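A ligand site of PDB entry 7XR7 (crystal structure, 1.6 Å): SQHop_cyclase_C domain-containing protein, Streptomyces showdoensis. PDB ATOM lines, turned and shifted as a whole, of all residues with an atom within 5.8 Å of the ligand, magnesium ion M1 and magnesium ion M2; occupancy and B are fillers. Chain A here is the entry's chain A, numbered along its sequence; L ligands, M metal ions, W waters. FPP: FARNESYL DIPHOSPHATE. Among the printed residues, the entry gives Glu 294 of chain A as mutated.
The backbone nitrogen of Pro 491 lies close to an oxygen (O1A) of the ligand (3.5 Å).
Phe 239 touches the ligand (CE2 to C3, 3.7 Å).
Ile 240 touches the ligand.
Met 243 touches the ligand (CE to C14, 3.6 Å).
Phe 246 touches the ligand.
Phe 284 touches the ligand.
Asp 292 touches the ligand (OD1 to C10, 3.6 Å).
OE1 of Glu 294 touches C12 of the ligand, at 3.2 Å.
Asp 295 touches the ligand (OD2 to C15, 3.4 Å).
Thr 334 touches the ligand.
Phe 335 touches the ligand (CZ to C9, 3.9 Å).
Trp 384 touches the ligand (CZ3 to O1, 3.4 Å).
OE1 of Gln 488 touches C14 of the ligand, at 3.1 Å.
Gly 490 touches the ligand (CA to O1, 3.9 Å).
Tyr 496 touches the ligand (OH to C5, 3.1 Å).
Hydrophobic or aromatic side chains within 4 Å of the ligand: Trp 156, Phe 239, Ile 240, Met 243, Phe 246, Phe 284, Phe 335, Trp 384, Pro 491 and Tyr 496.
Of the 31 residues printed, 20 come within 4 Å of the ligand.
Magnesium ion M1 is bound by the side-chain carboxylate (OE2) of Glu 160 and an oxygen (O1A) of the ligand.
The side-chain amide nitrogen (NE2) of Gln 154 is in hydrogen-bond range of an oxygen (O2A) of the ligand (2.5 Å).
The side-chain amino group (NZ) of Lys 124 is in salt-bridge range of an oxygen (O2B) of the ligand, at 2.6 Å.
The guanidinium group (NH1) of Arg 123 lies within salt-bridge range of an oxygen (O3B) of the ligand (2.9 Å).
O2A of the ligand sits at hydrogen-bond distance from NE1 of Trp 156, at 2.9 Å.
The backbone NH (N) of Arg 492 lies within hydrogen-bond range of an oxygen (O2B) of the ligand, at 2.9 Å.
The guanidinium group (NE) of Arg 492 is in salt-bridge range of an oxygen (O2B) of the ligand, 2.9 Å away.
Magnesium ion M2 is bound by the side-chain carboxylate of Glu 160 (2.5 Å).
Slightly farther from magnesium ion M2 lies O3B of the ligand (2.7 Å).
Slightly farther from magnesium ion M2 lies O1A of the ligand (2.8 Å).
Water W1 lies within hydrogen-bond range of the side-chain carboxylate (OD1) of Asp 292 (2.7 Å) and the backbone NH (N) of Phe 284 (3.4 Å).
Merely in contact with magnesium ion M1: Asn 199, Phe 239, Trp 156 and Leu 201.
Five residues have an atom within 4 Å of magnesium ion M1: Trp 156, Glu 160, Asn 199, Leu 201 and Phe 239.
The backbone NH (N) of Tyr 496 sits at hydrogen-bond distance from the backbone carbonyl oxygen (O) of Gln 488, 3.0 Å away.
OE1 of Gln 488 sits close to O of Trp 384, 3.4 Å away.
The backbone NH (N) of Glu 294 sits at hydrogen-bond distance from the side-chain sulfur (SD) of Met 345.
NE1 of Trp 384 is in hydrogen-bond range of OG1 of Thr 334.
The backbone NH (N) of Ala 489 sits at hydrogen-bond distance from the backbone carbonyl oxygen (O) of Trp 384.
OD2 of Asp 295 lies close to N of Phe 284 (3.3 Å).
N of Asp 295 sits at hydrogen-bond distance from OD2 of Asp 292 (2.8 Å).
O of Phe 284 sits at hydrogen-bond distance from N of Phe 246, 3.3 Å away.
Leu 157 touches magnesium ion M2 (CD1 to MG, 3.7 Å).
Pro 491 touches magnesium ion M2.
Of the 31 residues printed, 3 come within 4 Å of magnesium ion M2.
Along chain A the residues within 4 Å of magnesium ion M2 span positions 157 to 491.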
ATOM      1  N   HIS A 118     -23.838  36.214 -33.567  1.00  0.00           N
ATOM      2  CA  HIS A 118     -23.465  35.650 -32.277  1.00  0.00           C
ATOM      3  C   HIS A 118     -21.966  35.819 -32.079  1.00  0.00           C
ATOM      4  O   HIS A 118     -21.199  35.862 -33.043  1.00  0.00           O
ATOM      5  CB  HIS A 118     -23.854  34.162 -32.204  1.00  0.00           C
ATOM      6  CG  HIS A 118     -23.869  33.608 -30.822  1.00  0.00           C
ATOM      7  ND1 HIS A 118     -22.869  32.791 -30.337  1.00  0.00           N
ATOM      8  CD2 HIS A 118     -24.762  33.738 -29.812  1.00  0.00           C
ATOM      9  CE1 HIS A 118     -23.153  32.445 -29.084  1.00  0.00           C
ATOM     10  NE2 HIS A 118     -24.299  33.008 -28.748  1.00  0.00           N
ATOM     11  N   THR A 120     -19.829  33.781 -31.162  1.00  0.00           N
ATOM     12  CA  THR A 120     -19.053  32.611 -31.558  1.00  0.00           C
ATOM     13  C   THR A 120     -18.949  32.447 -33.079  1.00  0.00           C
ATOM     14  O   THR A 120     -18.422  31.439 -33.537  1.00  0.00           O
ATOM     15  CB  THR A 120     -19.645  31.340 -30.954  1.00  0.00           C
ATOM     16  OG1 THR A 120     -20.943  31.098 -31.505  1.00  0.00           O
ATOM     17  CG2 THR A 120     -19.759  31.460 -29.435  1.00  0.00           C
ATOM     18  N   ARG A 123     -15.416  31.493 -34.526  1.00  0.00           N
ATOM     19  CA  ARG A 123     -15.042  30.112 -34.221  1.00  0.00           C
ATOM     20  C   ARG A 123     -15.864  29.126 -35.046  1.00  0.00           C
ATOM     21  O   ARG A 123     -15.321  28.130 -35.550  1.00  0.00           O
ATOM     22  CB  ARG A 123     -15.230  29.841 -32.722  1.00  0.00           C
ATOM     23  CG  ARG A 123     -15.274  28.360 -32.347  1.00  0.00           C
ATOM     24  CD  ARG A 123     -15.053  28.152 -30.856  1.00  0.00           C
ATOM     25  NE  ARG A 123     -16.135  28.651 -30.016  1.00  0.00           N
ATOM     26  CZ  ARG A 123     -17.238  27.980 -29.744  1.00  0.00           C
ATOM     27  NH1 ARG A 123     -17.495  26.794 -30.288  1.00  0.00           N
ATOM     28  NH2 ARG A 123     -18.126  28.508 -28.904  1.00  0.00           N
ATOM     29  N   LYS A 124     -17.165  29.386 -35.200  1.00  0.00           N
ATOM     30  CA  LYS A 124     -18.016  28.449 -35.930  1.00  0.00           C
ATOM     31  C   LYS A 124     -17.602  28.352 -37.389  1.00  0.00           C
ATOM     32  O   LYS A 124     -17.619  27.265 -37.974  1.00  0.00           O
ATOM     33  CB  LYS A 124     -19.481  28.876 -35.820  1.00  0.00           C
ATOM     34  CG  LYS A 124     -20.028  28.765 -34.416  1.00  0.00           C
ATOM     35  CD  LYS A 124     -19.936  27.340 -33.915  1.00  0.00           C
ATOM     36  CE  LYS A 124     -20.094  27.301 -32.407  1.00  0.00           C
ATOM     37  NZ  LYS A 124     -21.265  28.089 -31.970  1.00  0.00           N
ATOM     38  N   MET A 127     -14.625  26.090 -37.350  1.00  0.00           N
ATOM     39  CA  MET A 127     -15.050  24.733 -37.028  1.00  0.00           C
ATOM     40  C   MET A 127     -15.757  24.080 -38.218  1.00  0.00           C
ATOM     41  O   MET A 127     -15.406  22.967 -38.622  1.00  0.00           O
ATOM     42  CB  MET A 127     -15.995  24.730 -35.830  1.00  0.00           C
ATOM     43  CG  MET A 127     -15.357  24.950 -34.474  1.00  0.00           C
ATOM     44  SD  MET A 127     -16.643  24.915 -33.212  1.00  0.00           S
ATOM     45  CE  MET A 127     -17.669  23.574 -33.829  1.00  0.00           C
ATOM     46  N   GLN A 154     -16.575  25.347 -21.942  1.00  0.00           N
ATOM     47  CA  GLN A 154     -17.177  24.040 -21.727  1.00  0.00           C
ATOM     48  C   GLN A 154     -16.136  22.959 -21.994  1.00  0.00           C
ATOM     49  O   GLN A 154     -15.314  23.088 -22.917  1.00  0.00           O
ATOM     50  CB  GLN A 154     -18.411  23.815 -22.609  1.00  0.00           C
ATOM     51  CG  GLN A 154     -18.150  23.911 -24.105  1.00  0.00           C
ATOM     52  CD  GLN A 154     -18.499  25.273 -24.670  1.00  0.00           C
ATOM     53  OE1 GLN A 154     -17.974  26.285 -24.224  1.00  0.00           O
ATOM     54  NE2 GLN A 154     -19.397  25.296 -25.659  1.00  0.00           N
ATOM     55  N   TRP A 156     -15.966  19.985 -23.260  1.00  0.00           N
ATOM     56  CA  TRP A 156     -15.850  19.267 -24.522  1.00  0.00           C
ATOM     57  C   TRP A 156     -15.429  20.171 -25.678  1.00  0.00           C
ATOM     58  O   TRP A 156     -14.924  19.658 -26.684  1.00  0.00           O
ATOM     59  CB  TRP A 156     -17.185  18.591 -24.839  1.00  0.00           C
ATOM     60  CG  TRP A 156     -18.360  19.536 -24.831  1.00  0.00           C
ATOM     61  CD1 TRP A 156     -18.793  20.299 -25.870  1.00  0.00           C
ATOM     62  CD2 TRP A 156     -19.239  19.807 -23.732  1.00  0.00           C
ATOM     63  NE1 TRP A 156     -19.896  21.035 -25.496  1.00  0.00           N
ATOM     64  CE2 TRP A 156     -20.188  20.757 -24.191  1.00  0.00           C
ATOM     65  CE3 TRP A 156     -19.330  19.344 -22.413  1.00  0.00           C
ATOM     66  CZ2 TRP A 156     -21.212  21.242 -23.373  1.00  0.00           C
ATOM     67  CZ3 TRP A 156     -20.334  19.834 -21.604  1.00  0.00           C
ATOM     68  CH2 TRP A 156     -21.266  20.771 -22.086  1.00  0.00           C
ATOM     69  N   LEU A 157     -15.606  21.485 -25.572  1.00  0.00           N
ATOM     70  CA  LEU A 157     -15.255  22.371 -26.681  1.00  0.00           C
ATOM     71  C   LEU A 157     -13.751  22.410 -26.908  1.00  0.00           C
ATOM     72  O   LEU A 157     -13.288  22.499 -28.048  1.00  0.00           O
ATOM     73  CB  LEU A 157     -15.786  23.777 -26.433  1.00  0.00           C
ATOM     74  CG  LEU A 157     -15.259  24.809 -27.438  1.00  0.00           C
ATOM     75  CD1 LEU A 157     -15.791  24.532 -28.843  1.00  0.00           C
ATOM     76  CD2 LEU A 157     -15.593  26.226 -26.995  1.00  0.00           C
ATOM     77  N   GLU A 160     -13.139  19.418 -29.064  1.00  0.00           N
ATOM     78  CA  GLU A 160     -13.550  19.581 -30.453  1.00  0.00           C
ATOM     79  C   GLU A 160     -12.536  20.394 -31.247  1.00  0.00           C
ATOM     80  O   GLU A 160     -12.150  20.022 -32.362  1.00  0.00           O
ATOM     81  CB  GLU A 160     -14.932  20.240 -30.535  1.00  0.00           C
ATOM     82  CG  GLU A 160     -16.036  19.415 -29.889  1.00  0.00           C
ATOM     83  CD  GLU A 160     -17.290  20.214 -29.688  1.00  0.00           C
ATOM     84  OE1 GLU A 160     -17.183  21.461 -29.578  1.00  0.00           O
ATOM     85  OE2 GLU A 160     -18.376  19.617 -29.647  1.00  0.00           O
ATOM     86  N   GLU A 197     -19.050  13.350 -21.164  1.00  0.00           N
ATOM     87  CA  GLU A 197     -19.955  14.497 -21.080  1.00  0.00           C
ATOM     88  C   GLU A 197     -21.198  14.311 -21.951  1.00  0.00           C
ATOM     89  O   GLU A 197     -21.855  15.299 -22.315  1.00  0.00           O
ATOM     90  CB  GLU A 197     -19.242  15.806 -21.445  1.00  0.00           C
ATOM     91  CG  GLU A 197     -18.094  16.146 -20.505  1.00  0.00           C
ATOM     92  CD  GLU A 197     -18.570  16.501 -19.103  1.00  0.00           C
ATOM     93  OE1 GLU A 197     -18.892  15.575 -18.322  1.00  0.00           O
ATOM     94  OE2 GLU A 197     -18.638  17.700 -18.797  1.00  0.00           O
ATOM     95  N   ASN A 199     -21.600  13.711 -24.978  1.00  0.00           N
ATOM     96  CA  ASN A 199     -21.515  14.494 -26.213  1.00  0.00           C
ATOM     97  C   ASN A 199     -20.917  13.639 -27.321  1.00  0.00           C
ATOM     98  O   ASN A 199     -19.706  13.459 -27.398  1.00  0.00           O
ATOM     99  CB  ASN A 199     -20.698  15.765 -25.972  1.00  0.00           C
ATOM    100  CG  ASN A 199     -20.756  16.706 -27.133  1.00  0.00           C
ATOM    101  OD1 ASN A 199     -20.714  16.293 -28.294  1.00  0.00           O
ATOM    102  ND2 ASN A 199     -20.862  18.003 -26.847  1.00  0.00           N
ATOM    103  N   LEU A 201     -20.901  14.269 -30.586  1.00  0.00           N
ATOM    104  CA  LEU A 201     -20.158  15.035 -31.586  1.00  0.00           C
ATOM    105  C   LEU A 201     -18.698  15.159 -31.191  1.00  0.00           C
ATOM    106  O   LEU A 201     -17.799  14.912 -31.994  1.00  0.00           O
ATOM    107  CB  LEU A 201     -20.795  16.412 -31.776  1.00  0.00           C
ATOM    108  CG  LEU A 201     -20.002  17.390 -32.647  1.00  0.00           C
ATOM    109  CD1 LEU A 201     -19.830  16.849 -34.059  1.00  0.00           C
ATOM    110  CD2 LEU A 201     -20.711  18.751 -32.683  1.00  0.00           C
ATOM    111  N   ALA A 202     -18.436  15.538 -29.934  1.00  0.00           N
ATOM    112  CA  ALA A 202     -17.064  15.710 -29.497  1.00  0.00           C
ATOM    113  C   ALA A 202     -16.292  14.394 -29.584  1.00  0.00           C
ATOM    114  O   ALA A 202     -15.147  14.379 -30.025  1.00  0.00           O
ATOM    115  CB  ALA A 202     -17.016  16.255 -28.065  1.00  0.00           C
ATOM    116  N   PHE A 239     -27.012  13.715 -31.187  1.00  0.00           N
ATOM    117  CA  PHE A 239     -25.992  14.663 -30.757  1.00  0.00           C
ATOM    118  C   PHE A 239     -25.533  14.354 -29.338  1.00  0.00           C
ATOM    119  O   PHE A 239     -24.328  14.275 -29.061  1.00  0.00           O
ATOM    120  CB  PHE A 239     -26.552  16.083 -30.869  1.00  0.00           C
ATOM    121  CG  PHE A 239     -25.731  17.157 -30.175  1.00  0.00           C
ATOM    122  CD1 PHE A 239     -24.346  17.158 -30.220  1.00  0.00           C
ATOM    123  CD2 PHE A 239     -26.371  18.189 -29.512  1.00  0.00           C
ATOM    124  CE1 PHE A 239     -23.621  18.158 -29.588  1.00  0.00           C
ATOM    125  CE2 PHE A 239     -25.648  19.186 -28.897  1.00  0.00           C
ATOM    126  CZ  PHE A 239     -24.263  19.173 -28.939  1.00  0.00           C
ATOM    127  N   ILE A 240     -26.484  14.179 -28.414  1.00  0.00           N
ATOM    128  CA  ILE A 240     -26.208  13.925 -27.002  1.00  0.00           C
ATOM    129  C   ILE A 240     -27.055  12.751 -26.530  1.00  0.00           C
ATOM    130  O   ILE A 240     -28.022  12.343 -27.169  1.00  0.00           O
ATOM    131  CB  ILE A 240     -26.485  15.161 -26.127  1.00  0.00           C
ATOM    132  CG1 ILE A 240     -27.894  15.683 -26.392  1.00  0.00           C
ATOM    133  CG2 ILE A 240     -25.427  16.249 -26.382  1.00  0.00           C
ATOM    134  CD1 ILE A 240     -28.265  16.903 -25.544  1.00  0.00           C
ATOM    135  N   MET A 243     -31.208  15.001 -22.288  1.00  0.00           N
ATOM    136  CA  MET A 243     -31.200  16.235 -21.518  1.00  0.00           C
ATOM    137  C   MET A 243     -32.085  16.090 -20.293  1.00  0.00           C
ATOM    138  O   MET A 243     -32.919  16.957 -20.013  1.00  0.00           O
ATOM    139  CB  MET A 243     -31.683  17.421 -22.363  1.00  0.00           C
ATOM    140  CG  MET A 243     -30.678  18.075 -23.266  1.00  0.00           C
ATOM    141  SD  MET A 243     -31.542  19.495 -23.988  1.00  0.00           S
ATOM    142  CE  MET A 243     -30.843  20.867 -23.061  1.00  0.00           C
ATOM    143  N   PHE A 246     -31.983  19.080 -17.426  1.00  0.00           N
ATOM    144  CA  PHE A 246     -32.680  20.268 -17.915  1.00  0.00           C
ATOM    145  C   PHE A 246     -34.183  20.029 -17.962  1.00  0.00           C
ATOM    146  O   PHE A 246     -34.973  20.848 -17.482  1.00  0.00           O
ATOM    147  CB  PHE A 246     -32.139  20.607 -19.304  1.00  0.00           C
ATOM    148  CG  PHE A 246     -32.701  21.859 -19.916  1.00  0.00           C
ATOM    149  CD1 PHE A 246     -32.233  23.110 -19.547  1.00  0.00           C
ATOM    150  CD2 PHE A 246     -33.655  21.781 -20.914  1.00  0.00           C
ATOM    151  CE1 PHE A 246     -32.740  24.264 -20.134  1.00  0.00           C
ATOM    152  CE2 PHE A 246     -34.162  22.935 -21.501  1.00  0.00           C
ATOM    153  CZ  PHE A 246     -33.697  24.168 -21.117  1.00  0.00           C
ATOM    154  N   PHE A 284     -26.489  19.201 -18.058  1.00  0.00           N
ATOM    155  CA  PHE A 284     -27.757  19.042 -18.766  1.00  0.00           C
ATOM    156  C   PHE A 284     -28.329  17.623 -18.703  1.00  0.00           C
ATOM    157  O   PHE A 284     -29.525  17.440 -18.952  1.00  0.00           O
ATOM    158  CB  PHE A 284     -27.602  19.485 -20.237  1.00  0.00           C
ATOM    159  CG  PHE A 284     -26.631  18.653 -21.032  1.00  0.00           C
ATOM    160  CD1 PHE A 284     -27.042  17.501 -21.683  1.00  0.00           C
ATOM    161  CD2 PHE A 284     -25.319  19.063 -21.169  1.00  0.00           C
ATOM    162  CE1 PHE A 284     -26.144  16.740 -22.424  1.00  0.00           C
ATOM    163  CE2 PHE A 284     -24.421  18.330 -21.916  1.00  0.00           C
ATOM    164  CZ  PHE A 284     -24.825  17.161 -22.540  1.00  0.00           C
ATOM    165  N   ASP A 292     -23.639  24.392 -16.001  1.00  0.00           N
ATOM    166  CA  ASP A 292     -23.930  25.592 -16.783  1.00  0.00           C
ATOM    167  C   ASP A 292     -25.024  26.386 -16.090  1.00  0.00           C
ATOM    168  O   ASP A 292     -25.790  25.870 -15.285  1.00  0.00           O
ATOM    169  CB  ASP A 292     -24.349  25.242 -18.210  1.00  0.00           C
ATOM    170  CG  ASP A 292     -25.700  24.572 -18.254  1.00  0.00           C
ATOM    171  OD1 ASP A 292     -25.728  23.320 -18.164  1.00  0.00           O
ATOM    172  OD2 ASP A 292     -26.721  25.284 -18.335  1.00  0.00           O
ATOM    173  N   GLU A 294     -27.806  27.819 -17.288  1.00  0.00           N
ATOM    174  CA  GLU A 294     -29.205  27.566 -17.629  1.00  0.00           C
ATOM    175  C   GLU A 294     -29.776  26.410 -16.814  1.00  0.00           C
ATOM    176  O   GLU A 294     -30.841  26.539 -16.186  1.00  0.00           O
ATOM    177  CB  GLU A 294     -29.348  27.292 -19.129  1.00  0.00           C
ATOM    178  CG  GLU A 294     -30.806  27.104 -19.553  1.00  0.00           C
ATOM    179  CD  GLU A 294     -31.148  27.835 -20.833  1.00  0.00           C
ATOM    180  OE1 GLU A 294     -30.277  27.964 -21.715  1.00  0.00           O
ATOM    181  OE2 GLU A 294     -32.306  28.306 -20.951  1.00  0.00           O
ATOM    182  N   ASP A 295     -29.104  25.255 -16.839  1.00  0.00           N
ATOM    183  CA  ASP A 295     -29.537  24.129 -16.027  1.00  0.00           C
ATOM    184  C   ASP A 295     -29.634  24.514 -14.552  1.00  0.00           C
ATOM    185  O   ASP A 295     -30.620  24.189 -13.878  1.00  0.00           O
ATOM    186  CB  ASP A 295     -28.562  22.960 -16.210  1.00  0.00           C
ATOM    187  CG  ASP A 295     -28.815  22.201 -17.486  1.00  0.00           C
ATOM    188  OD1 ASP A 295     -29.900  21.591 -17.579  1.00  0.00           O
ATOM    189  OD2 ASP A 295     -27.945  22.196 -18.382  1.00  0.00           O
ATOM    190  N   THR A 334     -22.514  31.438 -19.981  1.00  0.00           N
ATOM    191  CA  THR A 334     -23.156  30.131 -19.874  1.00  0.00           C
ATOM    192  C   THR A 334     -22.352  29.172 -18.993  1.00  0.00           C
ATOM    193  O   THR A 334     -22.937  28.452 -18.163  1.00  0.00           O
ATOM    194  CB  THR A 334     -23.340  29.493 -21.253  1.00  0.00           C
ATOM    195  OG1 THR A 334     -24.149  30.341 -22.081  1.00  0.00           O
ATOM    196  CG2 THR A 334     -24.006  28.124 -21.142  1.00  0.00           C
ATOM    197  N   PHE A 335     -21.029  29.138 -19.179  1.00  0.00           N
ATOM    198  CA  PHE A 335     -20.176  28.092 -18.606  1.00  0.00           C
ATOM    199  C   PHE A 335     -19.052  28.617 -17.724  1.00  0.00           C
ATOM    200  O   PHE A 335     -18.733  27.991 -16.711  1.00  0.00           O
ATOM    201  CB  PHE A 335     -19.503  27.275 -19.731  1.00  0.00           C
ATOM    202  CG  PHE A 335     -20.456  26.479 -20.567  1.00  0.00           C
ATOM    203  CD1 PHE A 335     -21.125  25.374 -20.046  1.00  0.00           C
ATOM    204  CD2 PHE A 335     -20.624  26.773 -21.910  1.00  0.00           C
ATOM    205  CE1 PHE A 335     -21.971  24.614 -20.831  1.00  0.00           C
ATOM    206  CE2 PHE A 335     -21.475  26.019 -22.702  1.00  0.00           C
ATOM    207  CZ  PHE A 335     -22.153  24.952 -22.170  1.00  0.00           C
ATOM    208  N   MET A 345     -28.927  34.228 -20.176  1.00  0.00           N
ATOM    209  CA  MET A 345     -28.326  33.692 -18.954  1.00  0.00           C
ATOM    210  C   MET A 345     -28.353  34.731 -17.837  1.00  0.00           C
ATOM    211  O   MET A 345     -28.572  34.394 -16.665  1.00  0.00           O
ATOM    212  CB  MET A 345     -26.878  33.248 -19.219  1.00  0.00           C
ATOM    213  CG  MET A 345     -26.703  32.165 -20.279  1.00  0.00           C
ATOM    214  SD  MET A 345     -27.475  30.595 -19.824  1.00  0.00           S
ATOM    215  CE  MET A 345     -29.116  30.826 -20.560  1.00  0.00           C
ATOM    216  N   TRP A 384     -28.853  29.763 -27.243  1.00  0.00           N
ATOM    217  CA  TRP A 384     -29.136  28.336 -27.171  1.00  0.00           C
ATOM    218  C   TRP A 384     -30.510  27.989 -27.722  1.00  0.00           C
ATOM    219  O   TRP A 384     -30.757  26.822 -28.027  1.00  0.00           O
ATOM    220  CB  TRP A 384     -29.001  27.861 -25.728  1.00  0.00           C
ATOM    221  CG  TRP A 384     -27.628  28.102 -25.168  1.00  0.00           C
ATOM    222  CD1 TRP A 384     -27.276  28.997 -24.198  1.00  0.00           C
ATOM    223  CD2 TRP A 384     -26.413  27.450 -25.572  1.00  0.00           C
ATOM    224  NE1 TRP A 384     -25.914  28.940 -23.962  1.00  0.00           N
ATOM    225  CE2 TRP A 384     -25.365  27.998 -24.798  1.00  0.00           C
ATOM    226  CE3 TRP A 384     -26.112  26.459 -26.511  1.00  0.00           C
ATOM    227  CZ2 TRP A 384     -24.045  27.580 -24.923  1.00  0.00           C
ATOM    228  CZ3 TRP A 384     -24.780  26.047 -26.639  1.00  0.00           C
ATOM    229  CH2 TRP A 384     -23.767  26.608 -25.846  1.00  0.00           C
ATOM    230  N   GLN A 488     -33.714  24.083 -29.700  1.00  0.00           N
ATOM    231  CA  GLN A 488     -32.398  24.039 -29.058  1.00  0.00           C
ATOM    232  C   GLN A 488     -31.298  23.904 -30.091  1.00  0.00           C
ATOM    233  O   GLN A 488     -31.432  23.167 -31.066  1.00  0.00           O
ATOM    234  CB  GLN A 488     -32.313  22.872 -28.074  1.00  0.00           C
ATOM    235  CG  GLN A 488     -33.334  22.909 -26.942  1.00  0.00           C
ATOM    236  CD  GLN A 488     -33.112  24.035 -25.961  1.00  0.00           C
ATOM    237  OE1 GLN A 488     -31.994  24.527 -25.801  1.00  0.00           O
ATOM    238  NE2 GLN A 488     -34.181  24.473 -25.306  1.00  0.00           N
ATOM    239  N   ALA A 489     -30.198  24.620 -29.867  1.00  0.00           N
ATOM    240  CA  ALA A 489     -29.060  24.626 -30.768  1.00  0.00           C
ATOM    241  C   ALA A 489     -27.790  24.235 -30.033  1.00  0.00           C
ATOM    242  O   ALA A 489     -27.644  24.497 -28.834  1.00  0.00           O
ATOM    243  CB  ALA A 489     -28.853  26.005 -31.408  1.00  0.00           C
ATOM    244  N   GLY A 490     -26.890  23.597 -30.770  1.00  0.00           N
ATOM    245  CA  GLY A 490     -25.609  23.207 -30.238  1.00  0.00           C
ATOM    246  C   GLY A 490     -24.916  22.214 -31.158  1.00  0.00           C
ATOM    247  O   GLY A 490     -25.511  21.209 -31.579  1.00  0.00           O
ATOM    248  N   PRO A 491     -23.690  22.525 -31.584  1.00  0.00           N
ATOM    249  CA  PRO A 491     -23.068  23.842 -31.502  1.00  0.00           C
ATOM    250  C   PRO A 491     -23.952  24.877 -32.169  1.00  0.00           C
ATOM    251  O   PRO A 491     -24.544  24.590 -33.209  1.00  0.00           O
ATOM    252  CB  PRO A 491     -21.772  23.689 -32.306  1.00  0.00           C
ATOM    253  CG  PRO A 491     -21.540  22.213 -32.386  1.00  0.00           C
ATOM    254  CD  PRO A 491     -22.886  21.577 -32.372  1.00  0.00           C
ATOM    255  N   ARG A 492     -24.077  26.045 -31.565  1.00  0.00           N
ATOM    256  CA  ARG A 492     -24.945  27.054 -32.145  1.00  0.00           C
ATOM    257  C   ARG A 492     -24.457  27.375 -33.560  1.00  0.00           C
ATOM    258  O   ARG A 492     -23.245  27.496 -33.787  1.00  0.00           O
ATOM    259  CB  ARG A 492     -24.945  28.304 -31.265  1.00  0.00           C
ATOM    260  CG  ARG A 492     -25.461  28.004 -29.857  1.00  0.00           C
ATOM    261  CD  ARG A 492     -25.089  29.089 -28.833  1.00  0.00           C
ATOM    262  NE  ARG A 492     -23.714  28.950 -28.362  1.00  0.00           N
ATOM    263  CZ  ARG A 492     -23.227  29.585 -27.297  1.00  0.00           C
ATOM    264  NH1 ARG A 492     -23.971  30.415 -26.581  1.00  0.00           N
ATOM    265  NH2 ARG A 492     -21.955  29.376 -26.942  1.00  0.00           N
ATOM    266  N   TYR A 496     -30.964  20.655 -32.596  1.00  0.00           N
ATOM    267  CA  TYR A 496     -31.113  19.247 -32.236  1.00  0.00           C
ATOM    268  C   TYR A 496     -32.452  19.091 -31.530  1.00  0.00           C
ATOM    269  O   TYR A 496     -33.013  20.073 -31.027  1.00  0.00           O
ATOM    270  CB  TYR A 496     -29.968  18.741 -31.339  1.00  0.00           C
ATOM    271  CG  TYR A 496     -29.869  19.430 -30.007  1.00  0.00           C
ATOM    272  CD1 TYR A 496     -30.551  18.944 -28.898  1.00  0.00           C
ATOM    273  CD2 TYR A 496     -29.077  20.554 -29.852  1.00  0.00           C
ATOM    274  CE1 TYR A 496     -30.453  19.578 -27.661  1.00  0.00           C
ATOM    275  CE2 TYR A 496     -28.967  21.193 -28.618  1.00  0.00           C
ATOM    276  CZ  TYR A 496     -29.665  20.708 -27.543  1.00  0.00           C
ATOM    277  OH  TYR A 496     -29.576  21.354 -26.320  1.00  0.00           O
HETATM  278  C1  FPP L   1     -23.385  21.915 -26.477  1.00  0.00           C
HETATM  279  O1  FPP L   1     -23.196  23.132 -27.206  1.00  0.00           O
HETATM  280  C2  FPP L   1     -24.813  21.774 -26.107  1.00  0.00           C
HETATM  281  C3  FPP L   1     -25.323  20.708 -25.507  1.00  0.00           C
HETATM  282  C4  FPP L   1     -24.515  19.511 -25.118  1.00  0.00           C
HETATM  283  C5  FPP L   1     -26.786  20.645 -25.149  1.00  0.00           C
HETATM  284  C6  FPP L   1     -27.126  21.367 -23.867  1.00  0.00           C
HETATM  285  C7  FPP L   1     -26.731  22.814 -23.861  1.00  0.00           C
HETATM  286  C8  FPP L   1     -26.089  23.479 -22.903  1.00  0.00           C
HETATM  287  C10 FPP L   1     -25.480  22.837 -21.707  1.00  0.00           C
HETATM  288  C9  FPP L   1     -25.941  24.972 -22.960  1.00  0.00           C
HETATM  289  C11 FPP L   1     -26.904  25.725 -22.060  1.00  0.00           C
HETATM  290  C12 FPP L   1     -28.328  25.603 -22.508  1.00  0.00           C
HETATM  291  C13 FPP L   1     -29.134  24.567 -22.376  1.00  0.00           C
HETATM  292  C14 FPP L   1     -30.375  24.397 -23.203  1.00  0.00           C
HETATM  293  C15 FPP L   1     -28.917  23.491 -21.355  1.00  0.00           C
HETATM  294  PA  FPP L   1     -21.736  23.477 -27.774  1.00  0.00           P
HETATM  295  O1A FPP L   1     -21.475  22.528 -28.906  1.00  0.00           O
HETATM  296  O2A FPP L   1     -20.796  23.510 -26.611  1.00  0.00           O
HETATM  297  O3A FPP L   1     -21.968  24.958 -28.341  1.00  0.00           O
HETATM  298  PB  FPP L   1     -21.075  26.176 -28.940  1.00  0.00           P
HETATM  299  O1B FPP L   1     -20.484  26.910 -27.764  1.00  0.00           O
HETATM  300  O2B FPP L   1     -22.056  27.005 -29.714  1.00  0.00           O
HETATM  301  O3B FPP L   1     -20.019  25.556 -29.812  1.00  0.00           O
HETATM  302 MG    MG M   1     -20.685  20.098 -28.962  1.00  0.00          MG
HETATM  303 MG    MG M   2     -18.978  23.083 -30.001  1.00  0.00          MG
HETATM  304  O   HOH W   1     -23.963  21.368 -18.929  1.00  0.00           O
HETATM  305  O   HOH W   2     -29.210  24.106 -26.466  1.00  0.00           O
